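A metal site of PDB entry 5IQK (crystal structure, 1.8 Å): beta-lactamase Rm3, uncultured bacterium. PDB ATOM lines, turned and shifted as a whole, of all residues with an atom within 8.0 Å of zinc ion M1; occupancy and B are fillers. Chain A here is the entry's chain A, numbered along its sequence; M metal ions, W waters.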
ATOM      1  N   TRP A  10      18.391 -11.974  29.977  1.00  0.00           N
ATOM      2  CA  TRP A  10      17.223 -12.620  29.384  1.00  0.00           C
ATOM      3  C   TRP A  10      17.600 -13.826  28.515  1.00  0.00           C
ATOM      4  O   TRP A  10      16.872 -14.821  28.475  1.00  0.00           O
ATOM      5  CB  TRP A  10      16.421 -11.628  28.555  1.00  0.00           C
ATOM      6  CG  TRP A  10      15.631 -10.623  29.391  1.00  0.00           C
ATOM      7  CD1 TRP A  10      15.565 -10.555  30.759  1.00  0.00           C
ATOM      8  CD2 TRP A  10      14.825  -9.554  28.896  1.00  0.00           C
ATOM      9  NE1 TRP A  10      14.744  -9.498  31.143  1.00  0.00           N
ATOM     10  CE2 TRP A  10      14.278  -8.880  30.012  1.00  0.00           C
ATOM     11  CE3 TRP A  10      14.509  -9.082  27.618  1.00  0.00           C
ATOM     12  CZ2 TRP A  10      13.432  -7.773  29.881  1.00  0.00           C
ATOM     13  CZ3 TRP A  10      13.672  -7.986  27.491  1.00  0.00           C
ATOM     14  CH2 TRP A  10      13.143  -7.351  28.616  1.00  0.00           C
ATOM     15  N   LEU A  31      13.448 -15.628  28.808  1.00  0.00           N
ATOM     16  CA  LEU A  31      12.541 -15.590  27.666  1.00  0.00           C
ATOM     17  C   LEU A  31      12.048 -16.997  27.327  1.00  0.00           C
ATOM     18  O   LEU A  31      12.871 -17.880  27.069  1.00  0.00           O
ATOM     19  CB  LEU A  31      13.252 -15.000  26.442  1.00  0.00           C
ATOM     20  CG  LEU A  31      13.789 -13.579  26.581  1.00  0.00           C
ATOM     21  CD1 LEU A  31      14.701 -13.252  25.410  1.00  0.00           C
ATOM     22  CD2 LEU A  31      12.629 -12.601  26.666  1.00  0.00           C
ATOM     23  N   SER A  76       3.638 -14.743  20.461  1.00  0.00           N
ATOM     24  CA  SER A  76       2.858 -14.105  21.509  1.00  0.00           C
ATOM     25  C   SER A  76       2.670 -12.617  21.164  1.00  0.00           C
ATOM     26  O   SER A  76       1.551 -12.155  20.965  1.00  0.00           O
ATOM     27  CB  SER A  76       3.539 -14.263  22.862  1.00  0.00           C
ATOM     28  OG  SER A  76       4.869 -13.774  22.810  1.00  0.00           O
ATOM     29  N   HIS A  77       3.772 -11.872  21.091  1.00  0.00           N
ATOM     30  CA  HIS A  77       3.681 -10.489  20.595  1.00  0.00           C
ATOM     31  C   HIS A  77       4.958 -10.052  19.865  1.00  0.00           C
ATOM     32  O   HIS A  77       5.974 -10.744  19.895  1.00  0.00           O
ATOM     33  CB  HIS A  77       3.320  -9.509  21.719  1.00  0.00           C
ATOM     34  CG  HIS A  77       4.367  -9.331  22.797  1.00  0.00           C
ATOM     35  ND1 HIS A  77       4.536 -10.235  23.826  1.00  0.00           N
ATOM     36  CD2 HIS A  77       5.219  -8.304  23.053  1.00  0.00           C
ATOM     37  CE1 HIS A  77       5.482  -9.800  24.645  1.00  0.00           C
ATOM     38  NE2 HIS A  77       5.913  -8.638  24.199  1.00  0.00           N
ATOM     39  N   GLY A  78       4.888  -8.872  19.242  1.00  0.00           N
ATOM     40  CA  GLY A  78       5.865  -8.463  18.250  1.00  0.00           C
ATOM     41  C   GLY A  78       7.149  -7.812  18.730  1.00  0.00           C
ATOM     42  O   GLY A  78       7.954  -7.346  17.933  1.00  0.00           O
ATOM     43  N   HIS A  79       7.337  -7.731  20.044  1.00  0.00           N
ATOM     44  CA  HIS A  79       8.597  -7.199  20.550  1.00  0.00           C
ATOM     45  C   HIS A  79       9.772  -8.082  20.185  1.00  0.00           C
ATOM     46  O   HIS A  79       9.613  -9.301  20.086  1.00  0.00           O
ATOM     47  CB  HIS A  79       8.537  -7.017  22.059  1.00  0.00           C
ATOM     48  CG  HIS A  79       7.758  -5.821  22.501  1.00  0.00           C
ATOM     49  ND1 HIS A  79       7.180  -5.744  23.741  1.00  0.00           N
ATOM     50  CD2 HIS A  79       7.472  -4.646  21.870  1.00  0.00           C
ATOM     51  CE1 HIS A  79       6.578  -4.567  23.879  1.00  0.00           C
ATOM     52  NE2 HIS A  79       6.731  -3.892  22.758  1.00  0.00           N
ATOM     53  N   ILE A  80      10.925  -7.451  20.018  1.00  0.00           N
ATOM     54  CA  ILE A  80      12.133  -8.147  19.585  1.00  0.00           C
ATOM     55  C   ILE A  80      12.534  -9.329  20.474  1.00  0.00           C
ATOM     56  O   ILE A  80      13.151 -10.282  19.986  1.00  0.00           O
ATOM     57  CB  ILE A  80      13.329  -7.135  19.480  1.00  0.00           C
ATOM     58  CG1 ILE A  80      14.569  -7.805  18.876  1.00  0.00           C
ATOM     59  CG2 ILE A  80      13.644  -6.515  20.846  1.00  0.00           C
ATOM     60  CD1 ILE A  80      15.620  -6.808  18.380  1.00  0.00           C
ATOM     61  N   ASP A  81      12.190  -9.296  21.754  1.00  0.00           N
ATOM     62  CA  ASP A  81      12.616 -10.378  22.639  1.00  0.00           C
ATOM     63  C   ASP A  81      11.719 -11.611  22.554  1.00  0.00           C
ATOM     64  O   ASP A  81      11.969 -12.593  23.272  1.00  0.00           O
ATOM     65  CB  ASP A  81      12.700  -9.901  24.104  1.00  0.00           C
ATOM     66  CG  ASP A  81      11.395  -9.292  24.605  1.00  0.00           C
ATOM     67  OD1 ASP A  81      10.774  -8.543  23.830  1.00  0.00           O
ATOM     68  OD2 ASP A  81      10.998  -9.550  25.772  1.00  0.00           O
ATOM     69  N   HIS A  82      10.688 -11.575  21.696  1.00  0.00           N
ATOM     70  CA  HIS A  82       9.846 -12.761  21.437  1.00  0.00           C
ATOM     71  C   HIS A  82       9.823 -13.090  19.940  1.00  0.00           C
ATOM     72  O   HIS A  82       9.646 -14.245  19.536  1.00  0.00           O
ATOM     73  CB  HIS A  82       8.427 -12.529  21.987  1.00  0.00           C
ATOM     74  CG  HIS A  82       8.418 -12.140  23.436  1.00  0.00           C
ATOM     75  ND1 HIS A  82       8.482 -13.072  24.453  1.00  0.00           N
ATOM     76  CD2 HIS A  82       8.444 -10.928  24.035  1.00  0.00           C
ATOM     77  CE1 HIS A  82       8.514 -12.449  25.618  1.00  0.00           C
ATOM     78  NE2 HIS A  82       8.488 -11.143  25.393  1.00  0.00           N
ATOM     79  N   ASP A 116       2.795   1.068  19.691  1.00  0.00           N
ATOM     80  CA  ASP A 116       3.472   0.221  20.658  1.00  0.00           C
ATOM     81  C   ASP A 116       4.001   1.062  21.816  1.00  0.00           C
ATOM     82  O   ASP A 116       4.584   2.136  21.593  1.00  0.00           O
ATOM     83  CB  ASP A 116       4.604  -0.557  19.998  1.00  0.00           C
ATOM     84  CG  ASP A 116       5.061  -1.742  20.835  1.00  0.00           C
ATOM     85  OD1 ASP A 116       4.733  -2.882  20.451  1.00  0.00           O
ATOM     86  OD2 ASP A 116       5.761  -1.537  21.857  1.00  0.00           O
ATOM     87  N   GLN A 118       6.535   0.656  23.346  1.00  0.00           N
ATOM     88  CA  GLN A 118       7.986   0.771  23.204  1.00  0.00           C
ATOM     89  C   GLN A 118       8.449   1.143  21.791  1.00  0.00           C
ATOM     90  O   GLN A 118       9.603   0.920  21.419  1.00  0.00           O
ATOM     91  CB  GLN A 118       8.647  -0.515  23.675  1.00  0.00           C
ATOM     92  CG  GLN A 118       8.299  -0.819  25.126  1.00  0.00           C
ATOM     93  CD  GLN A 118       8.973  -2.064  25.667  1.00  0.00           C
ATOM     94  OE1 GLN A 118       8.307  -2.949  26.209  1.00  0.00           O
ATOM     95  NE2 GLN A 118      10.295  -2.126  25.539  1.00  0.00           N
ATOM     96  N   LEU A 122      13.157   0.287  20.748  1.00  0.00           N
ATOM     97  CA  LEU A 122      13.671  -1.079  20.556  1.00  0.00           C
ATOM     98  C   LEU A 122      14.391  -1.171  19.214  1.00  0.00           C
ATOM     99  O   LEU A 122      14.052  -0.462  18.268  1.00  0.00           O
ATOM    100  CB  LEU A 122      12.536  -2.102  20.644  1.00  0.00           C
ATOM    101  CG  LEU A 122      11.913  -2.361  22.028  1.00  0.00           C
ATOM    102  CD1 LEU A 122      10.692  -3.266  21.945  1.00  0.00           C
ATOM    103  CD2 LEU A 122      12.929  -2.915  23.005  1.00  0.00           C
ATOM    104  N   HIS A 155      -0.064  -4.960  26.873  1.00  0.00           N
ATOM    105  CA  HIS A 155       1.378  -4.762  26.878  1.00  0.00           C
ATOM    106  C   HIS A 155       1.807  -4.339  25.469  1.00  0.00           C
ATOM    107  O   HIS A 155       2.727  -3.532  25.315  1.00  0.00           O
ATOM    108  CB  HIS A 155       2.084  -6.039  27.346  1.00  0.00           C
ATOM    109  CG  HIS A 155       3.560  -6.056  27.143  1.00  0.00           C
ATOM    110  ND1 HIS A 155       4.451  -5.498  28.042  1.00  0.00           N
ATOM    111  CD2 HIS A 155       4.323  -6.603  26.161  1.00  0.00           C
ATOM    112  CE1 HIS A 155       5.684  -5.674  27.617  1.00  0.00           C
ATOM    113  NE2 HIS A 155       5.639  -6.366  26.481  1.00  0.00           N
ATOM    114  N   THR A 156       1.140  -4.894  24.460  1.00  0.00           N
ATOM    115  CA  THR A 156       1.190  -4.403  23.069  1.00  0.00           C
ATOM    116  C   THR A 156      -0.220  -4.522  22.497  1.00  0.00           C
ATOM    117  O   THR A 156      -1.039  -5.264  23.044  1.00  0.00           O
ATOM    118  CB  THR A 156       2.162  -5.202  22.176  1.00  0.00           C
ATOM    119  OG1 THR A 156       1.656  -6.535  21.993  1.00  0.00           O
ATOM    120  CG2 THR A 156       3.560  -5.262  22.770  1.00  0.00           C
ATOM    121  N   ASP A 179       0.728 -14.514  27.284  1.00  0.00           N
ATOM    122  CA  ASP A 179       1.529 -13.400  26.838  1.00  0.00           C
ATOM    123  C   ASP A 179       1.806 -12.453  28.002  1.00  0.00           C
ATOM    124  O   ASP A 179       1.108 -12.457  29.018  1.00  0.00           O
ATOM    125  CB  ASP A 179       0.824 -12.636  25.708  1.00  0.00           C
ATOM    126  CG  ASP A 179       1.770 -11.681  25.003  1.00  0.00           C
ATOM    127  OD1 ASP A 179       3.012 -11.866  25.128  1.00  0.00           O
ATOM    128  OD2 ASP A 179       1.285 -10.742  24.347  1.00  0.00           O
ATOM    129  N   SER A 180       2.838 -11.639  27.842  1.00  0.00           N
ATOM    130  CA  SER A 180       3.070 -10.506  28.741  1.00  0.00           C
ATOM    131  C   SER A 180       1.827  -9.636  28.836  1.00  0.00           C
ATOM    132  O   SER A 180       1.233  -9.323  27.812  1.00  0.00           O
ATOM    133  CB  SER A 180       4.230  -9.641  28.242  1.00  0.00           C
ATOM    134  OG  SER A 180       5.421 -10.410  28.143  1.00  0.00           O
ATOM    135  N   ILE A 181       1.448  -9.263  30.057  1.00  0.00           N
ATOM    136  CA  ILE A 181       0.366  -8.314  30.286  1.00  0.00           C
ATOM    137  C   ILE A 181       0.807  -7.244  31.278  1.00  0.00           C
ATOM    138  O   ILE A 181      -0.022  -6.622  31.966  1.00  0.00           O
ATOM    139  CB  ILE A 181      -0.901  -9.016  30.810  1.00  0.00           C
ATOM    140  CG1 ILE A 181      -0.555  -9.931  31.983  1.00  0.00           C
ATOM    141  CG2 ILE A 181      -1.557  -9.824  29.693  1.00  0.00           C
ATOM    142  CD1 ILE A 181      -1.757 -10.511  32.685  1.00  0.00           C
ATOM    143  N   ASN A 182       2.124  -7.022  31.348  1.00  0.00           N
ATOM    144  CA  ASN A 182       2.644  -6.015  32.257  1.00  0.00           C
ATOM    145  C   ASN A 182       2.684  -4.639  31.589  1.00  0.00           C
ATOM    146  O   ASN A 182       3.161  -4.471  30.461  1.00  0.00           O
ATOM    147  CB  ASN A 182       4.036  -6.426  32.782  1.00  0.00           C
ATOM    148  CG  ASN A 182       5.077  -6.661  31.673  1.00  0.00           C
ATOM    149  OD1 ASN A 182       4.766  -7.126  30.578  1.00  0.00           O
ATOM    150  ND2 ASN A 182       6.331  -6.373  31.986  1.00  0.00           N
ATOM    151  N   VAL A 184       4.376  -1.915  31.105  1.00  0.00           N
ATOM    152  CA  VAL A 184       5.678  -1.275  31.046  1.00  0.00           C
ATOM    153  C   VAL A 184       5.833  -0.695  29.644  1.00  0.00           C
ATOM    154  O   VAL A 184       5.162  -1.139  28.696  1.00  0.00           O
ATOM    155  CB  VAL A 184       6.820  -2.265  31.326  1.00  0.00           C
ATOM    156  CG1 VAL A 184       6.620  -2.914  32.678  1.00  0.00           C
ATOM    157  CG2 VAL A 184       6.857  -3.338  30.238  1.00  0.00           C
ATOM    158  N   ALA A 222       5.306 -15.714  28.959  1.00  0.00           N
ATOM    159  CA  ALA A 222       6.273 -15.305  27.941  1.00  0.00           C
ATOM    160  C   ALA A 222       7.607 -14.932  28.571  1.00  0.00           C
ATOM    161  O   ALA A 222       8.670 -15.267  28.031  1.00  0.00           O
ATOM    162  CB  ALA A 222       5.709 -14.148  27.123  1.00  0.00           C
ATOM    163  N   HIS A 223       7.563 -14.259  29.711  1.00  0.00           N
ATOM    164  CA  HIS A 223       8.754 -14.108  30.558  1.00  0.00           C
ATOM    165  C   HIS A 223       8.605 -15.103  31.713  1.00  0.00           C
ATOM    166  O   HIS A 223       7.723 -14.916  32.555  1.00  0.00           O
ATOM    167  CB  HIS A 223       8.912 -12.661  31.066  1.00  0.00           C
ATOM    168  CG  HIS A 223       9.353 -11.691  30.018  1.00  0.00           C
ATOM    169  ND1 HIS A 223      10.630 -11.171  29.963  1.00  0.00           N
ATOM    170  CD2 HIS A 223       8.670 -11.136  28.980  1.00  0.00           C
ATOM    171  CE1 HIS A 223      10.723 -10.353  28.931  1.00  0.00           C
ATOM    172  NE2 HIS A 223       9.548 -10.308  28.326  1.00  0.00           N
HETATM  173 ZN    ZN M   1       7.003  -7.182  25.192  1.00  0.00          ZN
HETATM  174 ZN    ZN M   2       9.147  -9.585  26.478  1.00  0.00          ZN
HETATM  175  O   HOH W   1       7.122  -8.653  27.309  1.00  0.00           O
HETATM  176  O   HOH W   2       8.697  -7.595  25.949  1.00  0.00           O
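ND1 of His 155 sits at hydrogen-bond distance from O of Asn 182 (2.9 Å). A ring nitrogen (NE2) of His 79 lies within hydrogen-bond range of the side-chain carboxylate (OD2) of Asp 116. A ring nitrogen (ND1) of His 77 sits at hydrogen-bond distance from the side-chain carboxylate of Asp 179.
Of the 21 residues printed, 3 come within 4 Å of zinc ion M1. The nearest printed residue that does not touch zinc ion M1 is His 82 (4.2 Å).
Zinc ion M1 is bound by water W2 (1.9 Å), a ring nitrogen (NE2) of His 155 (2.0 Å), a ring nitrogen (ND1) of His 79 (2.1 Å), a ring nitrogen (NE2) of His 77 (2.1 Å) and water W1 (2.6 Å).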
